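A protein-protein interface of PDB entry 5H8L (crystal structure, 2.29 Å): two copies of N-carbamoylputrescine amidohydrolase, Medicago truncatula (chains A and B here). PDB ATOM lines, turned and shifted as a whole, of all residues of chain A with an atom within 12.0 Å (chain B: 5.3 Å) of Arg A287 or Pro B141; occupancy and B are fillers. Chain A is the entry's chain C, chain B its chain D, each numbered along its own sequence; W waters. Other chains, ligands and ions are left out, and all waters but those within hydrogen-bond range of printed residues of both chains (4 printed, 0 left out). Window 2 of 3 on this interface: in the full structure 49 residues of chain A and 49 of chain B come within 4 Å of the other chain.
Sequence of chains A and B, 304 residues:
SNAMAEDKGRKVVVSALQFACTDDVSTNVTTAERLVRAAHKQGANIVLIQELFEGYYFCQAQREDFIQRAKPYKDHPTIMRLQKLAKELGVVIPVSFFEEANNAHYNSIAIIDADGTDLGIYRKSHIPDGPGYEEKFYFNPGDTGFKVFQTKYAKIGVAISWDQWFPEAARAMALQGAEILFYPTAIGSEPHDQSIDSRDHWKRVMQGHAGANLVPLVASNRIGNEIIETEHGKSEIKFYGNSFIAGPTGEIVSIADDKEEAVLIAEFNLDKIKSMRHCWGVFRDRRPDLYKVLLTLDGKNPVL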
ATOM      1  N   ARG A 171      37.549  21.746  37.729  1.00  0.00           N
ATOM      2  CA  ARG A 171      36.274  22.164  37.178  1.00  0.00           C
ATOM      3  C   ARG A 171      35.192  22.141  38.247  1.00  0.00           C
ATOM      4  O   ARG A 171      34.372  23.062  38.344  1.00  0.00           O
ATOM      5  CB  ARG A 171      35.852  21.266  36.019  1.00  0.00           C
ATOM      6  CG  ARG A 171      34.562  21.719  35.349  1.00  0.00           C
ATOM      7  CD  ARG A 171      34.771  23.001  34.522  1.00  0.00           C
ATOM      8  NE  ARG A 171      34.914  22.696  33.099  1.00  0.00           N
ATOM      9  CZ  ARG A 171      35.400  23.544  32.199  1.00  0.00           C
ATOM     10  NH1 ARG A 171      35.931  24.661  32.582  1.00  0.00           N
ATOM     11  NH2 ARG A 171      35.455  23.201  30.934  1.00  0.00           N
ATOM     12  N   LEU A 175      33.116  25.417  39.092  1.00  0.00           N
ATOM     13  CA  LEU A 175      31.674  25.500  38.860  1.00  0.00           C
ATOM     14  C   LEU A 175      30.961  25.909  40.098  1.00  0.00           C
ATOM     15  O   LEU A 175      29.860  26.411  40.028  1.00  0.00           O
ATOM     16  CB  LEU A 175      31.099  24.164  38.414  1.00  0.00           C
ATOM     17  CG  LEU A 175      31.458  23.664  37.003  1.00  0.00           C
ATOM     18  CD1 LEU A 175      31.139  22.176  36.883  1.00  0.00           C
ATOM     19  CD2 LEU A 175      30.728  24.457  35.928  1.00  0.00           C
ATOM     20  N   ALA A 212      41.804  26.679  31.498  1.00  0.00           N
ATOM     21  CA  ALA A 212      40.495  26.122  31.039  1.00  0.00           C
ATOM     22  C   ALA A 212      39.335  26.618  31.880  1.00  0.00           C
ATOM     23  O   ALA A 212      38.166  26.629  31.410  1.00  0.00           O
ATOM     24  CB  ALA A 212      40.526  24.599  31.118  1.00  0.00           C
ATOM     25  N   ASN A 213      39.650  26.955  33.134  1.00  0.00           N
ATOM     26  CA  ASN A 213      38.697  27.529  34.062  1.00  0.00           C
ATOM     27  C   ASN A 213      38.817  29.036  34.253  1.00  0.00           C
ATOM     28  O   ASN A 213      37.999  29.619  34.953  1.00  0.00           O
ATOM     29  CB  ASN A 213      38.862  26.844  35.413  1.00  0.00           C
ATOM     30  CG  ASN A 213      38.439  25.412  35.338  1.00  0.00           C
ATOM     31  OD1 ASN A 213      37.245  25.122  35.227  1.00  0.00           O
ATOM     32  ND2 ASN A 213      39.422  24.488  35.294  1.00  0.00           N
ATOM     33  N   GLY A 281      33.737  32.649  27.796  1.00  0.00           N
ATOM     34  CA  GLY A 281      32.485  31.969  27.441  1.00  0.00           C
ATOM     35  C   GLY A 281      32.411  30.493  27.653  1.00  0.00           C
ATOM     36  O   GLY A 281      31.378  29.880  27.381  1.00  0.00           O
ATOM     37  N   VAL A 282      33.467  29.900  28.164  1.00  0.00           N
ATOM     38  CA  VAL A 282      33.467  28.458  28.248  1.00  0.00           C
ATOM     39  C   VAL A 282      32.366  27.939  29.158  1.00  0.00           C
ATOM     40  O   VAL A 282      31.757  26.883  28.890  1.00  0.00           O
ATOM     41  CB  VAL A 282      34.843  27.910  28.640  1.00  0.00           C
ATOM     42  CG1 VAL A 282      35.842  28.211  27.560  1.00  0.00           C
ATOM     43  CG2 VAL A 282      35.334  28.476  29.967  1.00  0.00           C
ATOM     44  N   PHE A 283      32.072  28.672  30.236  1.00  0.00           N
ATOM     45  CA  PHE A 283      31.079  28.160  31.191  1.00  0.00           C
ATOM     46  C   PHE A 283      29.657  28.308  30.601  1.00  0.00           C
ATOM     47  O   PHE A 283      28.725  27.642  31.009  1.00  0.00           O
ATOM     48  CB  PHE A 283      31.218  28.865  32.525  1.00  0.00           C
ATOM     49  CG  PHE A 283      32.386  28.400  33.322  1.00  0.00           C
ATOM     50  CD1 PHE A 283      32.323  27.228  34.063  1.00  0.00           C
ATOM     51  CD2 PHE A 283      33.572  29.132  33.348  1.00  0.00           C
ATOM     52  CE1 PHE A 283      33.422  26.791  34.796  1.00  0.00           C
ATOM     53  CE2 PHE A 283      34.661  28.683  34.076  1.00  0.00           C
ATOM     54  CZ  PHE A 283      34.583  27.514  34.817  1.00  0.00           C
ATOM     55  N   ARG A 284      29.511  29.203  29.635  1.00  0.00           N
ATOM     56  CA  ARG A 284      28.244  29.467  29.002  1.00  0.00           C
ATOM     57  C   ARG A 284      28.027  28.349  27.962  1.00  0.00           C
ATOM     58  O   ARG A 284      26.925  28.013  27.639  1.00  0.00           O
ATOM     59  CB  ARG A 284      28.303  30.850  28.293  1.00  0.00           C
ATOM     60  CG  ARG A 284      27.106  31.194  27.357  1.00  0.00           C
ATOM     61  CD  ARG A 284      27.495  32.237  26.333  1.00  0.00           C
ATOM     62  NE  ARG A 284      28.628  31.771  25.533  1.00  0.00           N
ATOM     63  CZ  ARG A 284      29.477  32.573  24.888  1.00  0.00           C
ATOM     64  NH1 ARG A 284      29.356  33.873  24.983  1.00  0.00           N
ATOM     65  NH2 ARG A 284      30.485  32.060  24.223  1.00  0.00           N
ATOM     66  N   ASP A 285      29.116  27.781  27.488  1.00  0.00           N
ATOM     67  CA  ASP A 285      29.110  26.857  26.378  1.00  0.00           C
ATOM     68  C   ASP A 285      29.222  25.371  26.796  1.00  0.00           C
ATOM     69  O   ASP A 285      29.169  24.500  25.949  1.00  0.00           O
ATOM     70  CB  ASP A 285      30.266  27.198  25.418  1.00  0.00           C
ATOM     71  CG  ASP A 285      30.135  28.603  24.796  1.00  0.00           C
ATOM     72  OD1 ASP A 285      29.032  29.169  24.872  1.00  0.00           O
ATOM     73  OD2 ASP A 285      31.166  29.161  24.238  1.00  0.00           O
ATOM     74  N   ARG A 286      29.408  25.076  28.067  1.00  0.00           N
ATOM     75  CA  ARG A 286      29.618  23.687  28.496  1.00  0.00           C
ATOM     76  C   ARG A 286      28.386  22.888  28.160  1.00  0.00           C
ATOM     77  O   ARG A 286      27.255  23.438  28.079  1.00  0.00           O
ATOM     78  CB  ARG A 286      29.892  23.609  30.002  1.00  0.00           C
ATOM     79  CG  ARG A 286      31.301  24.064  30.361  1.00  0.00           C
ATOM     80  CD  ARG A 286      31.637  23.883  31.849  1.00  0.00           C
ATOM     81  NE  ARG A 286      31.627  22.505  32.316  1.00  0.00           N
ATOM     82  CZ  ARG A 286      30.611  21.941  32.948  1.00  0.00           C
ATOM     83  NH1 ARG A 286      29.542  22.641  33.229  1.00  0.00           N
ATOM     84  NH2 ARG A 286      30.714  20.696  33.389  1.00  0.00           N
ATOM     85  N   ARG A 287      28.593  21.586  28.021  1.00  0.00           N
ATOM     86  CA  ARG A 287      27.539  20.635  27.595  1.00  0.00           C
ATOM     87  C   ARG A 287      27.380  19.450  28.595  1.00  0.00           C
ATOM     88  O   ARG A 287      27.726  18.294  28.305  1.00  0.00           O
ATOM     89  CB  ARG A 287      27.855  20.097  26.177  1.00  0.00           C
ATOM     90  CG  ARG A 287      27.849  21.138  25.070  1.00  0.00           C
ATOM     91  CD  ARG A 287      26.455  21.614  24.686  1.00  0.00           C
ATOM     92  NE  ARG A 287      25.516  20.551  24.493  1.00  0.00           N
ATOM     93  CZ  ARG A 287      25.353  19.889  23.359  1.00  0.00           C
ATOM     94  NH1 ARG A 287      26.102  20.170  22.314  1.00  0.00           N
ATOM     95  NH2 ARG A 287      24.406  18.959  23.261  1.00  0.00           N
ATOM     96  N   PRO A 288      26.804  19.718  29.754  1.00  0.00           N
ATOM     97  CA  PRO A 288      26.705  18.603  30.751  1.00  0.00           C
ATOM     98  C   PRO A 288      25.767  17.466  30.336  1.00  0.00           C
ATOM     99  O   PRO A 288      25.960  16.344  30.738  1.00  0.00           O
ATOM    100  CB  PRO A 288      26.270  19.329  32.055  1.00  0.00           C
ATOM    101  CG  PRO A 288      25.618  20.606  31.539  1.00  0.00           C
ATOM    102  CD  PRO A 288      26.458  21.018  30.347  1.00  0.00           C
ATOM    103  N   ASP A 289      24.797  17.755  29.503  1.00  0.00           N
ATOM    104  CA  ASP A 289      24.036  16.726  28.836  1.00  0.00           C
ATOM    105  C   ASP A 289      24.910  15.724  28.078  1.00  0.00           C
ATOM    106  O   ASP A 289      24.502  14.611  27.861  1.00  0.00           O
ATOM    107  CB  ASP A 289      23.001  17.354  27.881  1.00  0.00           C
ATOM    108  CG  ASP A 289      23.618  18.280  26.779  1.00  0.00           C
ATOM    109  OD1 ASP A 289      24.643  18.971  27.046  1.00  0.00           O
ATOM    110  OD2 ASP A 289      23.001  18.379  25.690  1.00  0.00           O
ATOM    111  N   LEU A 290      26.128  16.102  27.697  1.00  0.00           N
ATOM    112  CA  LEU A 290      26.965  15.203  26.960  1.00  0.00           C
ATOM    113  C   LEU A 290      28.060  14.627  27.843  1.00  0.00           C
ATOM    114  O   LEU A 290      28.931  13.905  27.359  1.00  0.00           O
ATOM    115  CB  LEU A 290      27.622  15.961  25.810  1.00  0.00           C
ATOM    116  CG  LEU A 290      26.704  16.495  24.740  1.00  0.00           C
ATOM    117  CD1 LEU A 290      27.472  17.049  23.539  1.00  0.00           C
ATOM    118  CD2 LEU A 290      25.702  15.430  24.264  1.00  0.00           C
ATOM    119  N   TYR A 291      28.059  14.956  29.128  1.00  0.00           N
ATOM    120  CA  TYR A 291      29.194  14.561  29.959  1.00  0.00           C
ATOM    121  C   TYR A 291      28.987  13.325  30.838  1.00  0.00           C
ATOM    122  O   TYR A 291      29.813  13.033  31.691  1.00  0.00           O
ATOM    123  CB  TYR A 291      29.676  15.711  30.855  1.00  0.00           C
ATOM    124  CG  TYR A 291      30.085  17.023  30.174  1.00  0.00           C
ATOM    125  CD1 TYR A 291      30.575  17.052  28.845  1.00  0.00           C
ATOM    126  CD2 TYR A 291      30.085  18.211  30.886  1.00  0.00           C
ATOM    127  CE1 TYR A 291      30.964  18.238  28.241  1.00  0.00           C
ATOM    128  CE2 TYR A 291      30.509  19.379  30.273  1.00  0.00           C
ATOM    129  CZ  TYR A 291      30.922  19.376  28.953  1.00  0.00           C
ATOM    130  OH  TYR A 291      31.315  20.537  28.383  1.00  0.00           O
ATOM    131  N   LYS A 292      27.929  12.585  30.632  1.00  0.00           N
ATOM    132  CA  LYS A 292      27.693  11.412  31.435  1.00  0.00           C
ATOM    133  C   LYS A 292      28.821  10.356  31.502  1.00  0.00           C
ATOM    134  O   LYS A 292      29.045   9.751  32.509  1.00  0.00           O
ATOM    135  CB  LYS A 292      26.425  10.770  30.996  1.00  0.00           C
ATOM    136  CG  LYS A 292      25.299  11.460  31.655  1.00  0.00           C
ATOM    137  CD  LYS A 292      23.969  10.988  31.145  1.00  0.00           C
ATOM    138  CE  LYS A 292      22.887  11.648  31.982  1.00  0.00           C
ATOM    139  NZ  LYS A 292      21.866  12.161  31.050  1.00  0.00           N
ATOM    140  N   VAL A 293      29.542  10.181  30.419  1.00  0.00           N
ATOM    141  CA  VAL A 293      30.573   9.235  30.359  1.00  0.00           C
ATOM    142  C   VAL A 293      31.643   9.586  31.383  1.00  0.00           C
ATOM    143  O   VAL A 293      32.411   8.721  31.801  1.00  0.00           O
ATOM    144  CB  VAL A 293      31.145   9.167  28.906  1.00  0.00           C
ATOM    145  CG1 VAL A 293      31.838  10.457  28.528  1.00  0.00           C
ATOM    146  CG2 VAL A 293      32.135   8.032  28.769  1.00  0.00           C
ATOM    147  N   LEU A 294      31.721  10.844  31.789  1.00  0.00           N
ATOM    148  CA  LEU A 294      32.664  11.157  32.820  1.00  0.00           C
ATOM    149  C   LEU A 294      32.353  10.430  34.157  1.00  0.00           C
ATOM    150  O   LEU A 294      33.210  10.353  35.039  1.00  0.00           O
ATOM    151  CB  LEU A 294      32.739  12.647  33.043  1.00  0.00           C
ATOM    152  CG  LEU A 294      33.184  13.551  31.881  1.00  0.00           C
ATOM    153  CD1 LEU A 294      33.299  14.972  32.397  1.00  0.00           C
ATOM    154  CD2 LEU A 294      34.535  13.191  31.371  1.00  0.00           C
ATOM    155  N   LEU A 295      31.134   9.930  34.320  1.00  0.00           N
ATOM    156  CA  LEU A 295      30.779   9.173  35.534  1.00  0.00           C
ATOM    157  C   LEU A 295      30.999   7.680  35.400  1.00  0.00           C
ATOM    158  O   LEU A 295      30.474   6.863  36.196  1.00  0.00           O
ATOM    159  CB  LEU A 295      29.340   9.388  35.938  1.00  0.00           C
ATOM    160  CG  LEU A 295      28.900  10.845  36.046  1.00  0.00           C
ATOM    161  CD1 LEU A 295      27.433  10.880  36.414  1.00  0.00           C
ATOM    162  CD2 LEU A 295      29.723  11.644  37.017  1.00  0.00           C
ATOM    163  N   TYR B 106      24.883  21.710  11.455  1.00  0.00           N
ATOM    164  CA  TYR B 106      25.960  21.419  12.354  1.00  0.00           C
ATOM    165  C   TYR B 106      27.272  21.655  11.759  1.00  0.00           C
ATOM    166  O   TYR B 106      27.427  21.647  10.537  1.00  0.00           O
ATOM    167  CB  TYR B 106      25.950  19.973  12.831  1.00  0.00           C
ATOM    168  CG  TYR B 106      24.647  19.444  13.364  1.00  0.00           C
ATOM    169  CD1 TYR B 106      24.328  19.517  14.726  1.00  0.00           C
ATOM    170  CD2 TYR B 106      23.770  18.784  12.518  1.00  0.00           C
ATOM    171  CE1 TYR B 106      23.109  18.977  15.207  1.00  0.00           C
ATOM    172  CE2 TYR B 106      22.583  18.243  12.975  1.00  0.00           C
ATOM    173  CZ  TYR B 106      22.248  18.325  14.327  1.00  0.00           C
ATOM    174  OH  TYR B 106      21.057  17.740  14.760  1.00  0.00           O
ATOM    175  N   LYS B 124      30.135  18.958  16.251  1.00  0.00           N
ATOM    176  CA  LYS B 124      30.722  19.857  17.205  1.00  0.00           C
ATOM    177  C   LYS B 124      29.800  20.124  18.380  1.00  0.00           C
ATOM    178  O   LYS B 124      28.707  20.626  18.165  1.00  0.00           O
ATOM    179  CB  LYS B 124      31.024  21.168  16.496  1.00  0.00           C
ATOM    180  CG  LYS B 124      31.894  22.119  17.277  1.00  0.00           C
ATOM    181  CD  LYS B 124      32.233  23.347  16.454  1.00  0.00           C
ATOM    182  CE  LYS B 124      33.159  24.267  17.239  1.00  0.00           C
ATOM    183  NZ  LYS B 124      33.834  25.319  16.381  1.00  0.00           N
ATOM    184  N   SER B 125      30.267  19.907  19.624  1.00  0.00           N
ATOM    185  CA  SER B 125      29.386  20.049  20.806  1.00  0.00           C
ATOM    186  C   SER B 125      29.318  21.429  21.431  1.00  0.00           C
ATOM    187  O   SER B 125      28.225  21.882  21.888  1.00  0.00           O
ATOM    188  CB  SER B 125      29.833  19.049  21.883  1.00  0.00           C
ATOM    189  OG  SER B 125      29.880  17.733  21.369  1.00  0.00           O
ATOM    190  N   HIS B 126      30.474  22.068  21.546  1.00  0.00           N
ATOM    191  CA  HIS B 126      30.590  23.356  22.160  1.00  0.00           C
ATOM    192  C   HIS B 126      30.713  24.405  21.054  1.00  0.00           C
ATOM    193  O   HIS B 126      31.615  24.346  20.240  1.00  0.00           O
ATOM    194  CB  HIS B 126      31.855  23.411  23.035  1.00  0.00           C
ATOM    195  CG  HIS B 126      31.921  22.344  24.087  1.00  0.00           C
ATOM    196  ND1 HIS B 126      32.641  21.190  23.922  1.00  0.00           N
ATOM    197  CD2 HIS B 126      31.418  22.292  25.343  1.00  0.00           C
ATOM    198  CE1 HIS B 126      32.515  20.432  25.001  1.00  0.00           C
ATOM    199  NE2 HIS B 126      31.785  21.085  25.883  1.00  0.00           N
ATOM    200  N   ILE B 127      29.819  25.372  21.053  1.00  0.00           N
ATOM    201  CA  ILE B 127      29.742  26.396  19.984  1.00  0.00           C
ATOM    202  C   ILE B 127      30.120  27.766  20.536  1.00  0.00           C
ATOM    203  O   ILE B 127      29.499  28.251  21.524  1.00  0.00           O
ATOM    204  CB  ILE B 127      28.318  26.499  19.408  1.00  0.00           C
ATOM    205  CG1 ILE B 127      27.711  25.116  19.250  1.00  0.00           C
ATOM    206  CG2 ILE B 127      28.328  27.196  18.041  1.00  0.00           C
ATOM    207  CD1 ILE B 127      28.528  24.179  18.394  1.00  0.00           C
ATOM    208  N   PHE B 139      25.036  27.037  13.989  1.00  0.00           N
ATOM    209  CA  PHE B 139      25.076  25.613  14.292  1.00  0.00           C
ATOM    210  C   PHE B 139      24.279  25.210  15.495  1.00  0.00           C
ATOM    211  O   PHE B 139      24.436  25.800  16.561  1.00  0.00           O
ATOM    212  CB  PHE B 139      26.513  25.168  14.588  1.00  0.00           C
ATOM    213  CG  PHE B 139      27.531  25.616  13.572  1.00  0.00           C
ATOM    214  CD1 PHE B 139      27.401  25.314  12.233  1.00  0.00           C
ATOM    215  CD2 PHE B 139      28.690  26.243  13.981  1.00  0.00           C
ATOM    216  CE1 PHE B 139      28.353  25.746  11.311  1.00  0.00           C
ATOM    217  CE2 PHE B 139      29.641  26.636  13.085  1.00  0.00           C
ATOM    218  CZ  PHE B 139      29.472  26.383  11.753  1.00  0.00           C
ATOM    219  N   ASN B 140      23.472  24.158  15.339  1.00  0.00           N
ATOM    220  CA  ASN B 140      22.849  23.520  16.484  1.00  0.00           C
ATOM    221  C   ASN B 140      23.973  22.974  17.313  1.00  0.00           C
ATOM    222  O   ASN B 140      24.931  22.476  16.781  1.00  0.00           O
ATOM    223  CB  ASN B 140      21.993  22.328  16.065  1.00  0.00           C
ATOM    224  CG  ASN B 140      20.665  22.748  15.444  1.00  0.00           C
ATOM    225  OD1 ASN B 140      20.584  23.113  14.264  1.00  0.00           O
ATOM    226  ND2 ASN B 140      19.598  22.679  16.259  1.00  0.00           N
ATOM    227  N   PRO B 141      23.886  23.090  18.628  1.00  0.00           N
ATOM    228  CA  PRO B 141      24.917  22.404  19.397  1.00  0.00           C
ATOM    229  C   PRO B 141      24.819  20.909  19.060  1.00  0.00           C
ATOM    230  O   PRO B 141      23.701  20.362  18.886  1.00  0.00           O
ATOM    231  CB  PRO B 141      24.517  22.663  20.840  1.00  0.00           C
ATOM    232  CG  PRO B 141      23.658  23.885  20.825  1.00  0.00           C
ATOM    233  CD  PRO B 141      22.902  23.752  19.499  1.00  0.00           C
ATOM    234  N   GLY B 142      25.994  20.287  18.937  1.00  0.00           N
ATOM    235  CA  GLY B 142      26.132  18.886  18.528  1.00  0.00           C
ATOM    236  C   GLY B 142      25.387  17.874  19.367  1.00  0.00           C
ATOM    237  O   GLY B 142      25.216  18.061  20.569  1.00  0.00           O
ATOM    238  N   ASP B 143      24.920  16.811  18.708  1.00  0.00           N
ATOM    239  CA  ASP B 143      24.124  15.819  19.387  1.00  0.00           C
ATOM    240  C   ASP B 143      24.618  14.390  19.162  1.00  0.00           C
ATOM    241  O   ASP B 143      23.928  13.446  19.523  1.00  0.00           O
ATOM    242  CB  ASP B 143      22.666  15.974  18.959  1.00  0.00           C
ATOM    243  CG  ASP B 143      22.507  15.942  17.461  1.00  0.00           C
ATOM    244  OD1 ASP B 143      23.474  15.546  16.773  1.00  0.00           O
ATOM    245  OD2 ASP B 143      21.415  16.281  16.986  1.00  0.00           O
ATOM    246  N   LEU B 297      25.534  23.219  35.222  1.00  0.00           N
ATOM    247  CA  LEU B 297      26.154  24.432  34.692  1.00  0.00           C
ATOM    248  C   LEU B 297      26.483  25.418  35.822  1.00  0.00           C
ATOM    249  O   LEU B 297      27.488  26.099  35.798  1.00  0.00           O
ATOM    250  CB  LEU B 297      25.198  25.134  33.721  1.00  0.00           C
ATOM    251  CG  LEU B 297      24.899  24.369  32.441  1.00  0.00           C
ATOM    252  CD1 LEU B 297      23.734  25.048  31.751  1.00  0.00           C
ATOM    253  CD2 LEU B 297      26.156  24.288  31.533  1.00  0.00           C
HETATM  254  O   HOH W   1      28.048  25.357  23.389  1.00  0.00           O
HETATM  255  O   HOH W   2      22.032  19.251  21.037  1.00  0.00           O
HETATM  256  O   HOH W   3      28.949  25.732  33.104  1.00  0.00           O
HETATM  257  O   HOH W   4      29.245  27.648  37.482  1.00  0.00           O
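Of the 11 printed residues of chain B, 6 touch a printed residue of chain A. Hydrophobic or aromatic side chains of chain B within 4 Å of the printed part of chain A: His B126, Pro B141 and Leu B297. Of the 19 printed residues of chain A, 7 touch a printed residue of chain B. Hydrophobic or aromatic side chains of chain A that line the printed part of chain B: Leu A175, Pro A288, Leu A290 and Tyr A291. Among the printed residues, no Asp or Glu carboxylate lies within 4 Å of a Lys or Arg side-chain nitrogen of the other chain.
O of Leu B297 touches CD2 of Leu A175, at 3.6 Å. Asp A285 touches His B126. Arg A286 touches His B126 (CA to CD2, 3.9 Å). Leu B297 touches Arg A286. His B126 touches Arg A287 (CD2 to CG, 3.8 Å). Arg A287 touches Pro B141. CD of Pro A288 touches CD2 of Leu B297, 3.5 Å away. Leu A290 touches Ser B125 (CD1 to OG, 3.3 Å). O of Gly B142 touches CD1 of Leu A290, 3.9 Å away.
Water W3 lies within hydrogen-bond range of O of Phe A283 (2.8 Å), O of Leu B297 (3.1 Å) and NH1 of Arg A286 (3.1 Å). Water W4 bridges O of Leu B297 and O of Leu A175. Water W1 lies within hydrogen-bond range of the backbone carbonyl oxygen of Asp A285 and the backbone NH of Ile B127. Water W2 lies within hydrogen-bond range of the backbone carbonyl oxygen of Pro B141 (2.9 Å), the guanidinium group of Arg A287 (3.3 Å) and the backbone carbonyl oxygen of Gly B142 (3.4 Å).
The guanidinium group (NH1) of Arg A287 sits at hydrogen-bond distance from the backbone carbonyl oxygen (O) of Ser B125. The backbone carbonyl oxygen (O) of Gly B142 sits at hydrogen-bond distance from the guanidinium group (NH1) of Arg A287 (2.9 Å). The side-chain hydroxyl (OH) of Tyr A291 is in hydrogen-bond range of a ring nitrogen (NE2) of His B126 (2.6 Å). OD2 of Asp A285 sits close to O of Ile B127, 3.3 Å away.
No position is printed for both chains.
The side-chain carboxylate (OD2) of Asp A289 is in salt-bridge range of the guanidinium group (NH2) of Arg A287 (2.9 Å). The side-chain hydroxyl of Tyr A291 is in hydrogen-bond range of the backbone NH of Arg A287. O of Lys B124 sits at hydrogen-bond distance from N of Gly B142 (2.8 Å). The guanidinium group of Arg A284 lies within salt-bridge range of the side-chain carboxylate of Asp A285 (2.7 Å).
Of the printed residues of chain B, Asp A285 touches His B126 (3.2 Å) and Ile B127 (3.3 Å). Printed residues of chain B within 4 Å of Arg A286: His B126 (3.9 Å) and Leu B297 (3.7 Å). Of the printed residues of chain B, Arg A287 touches Ser B125, His B126, Pro B141 and Gly B142. Printed residues of chain B within 4 Å of Pro A288: Leu B297. Printed residues of chain B within 4 Å of Tyr A291: His B126. Of chain A, only Arg A287 (2.8 Å) and Leu A290 (3.3 Å) come within 4 Å of Ser B125. His B126 touches four residues of chain A. Ile B127 touches just one residue of chain A: Asp A285. Of chain A, only Arg A287 (3.3 Å) comes within 4 Å of Pro B141. No residue of chain A comes within 4 Å of Asp B143. The nearest residue of chain B that does not touch Arg A287 is Lys B124 (4.9 Å). The nearest residue of chain A that does not touch Pro B141 is Leu A290 (6.5 Å). The nearest printed residue of chain A that does not touch Leu B297 is Phe A283 (4.3 Å).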
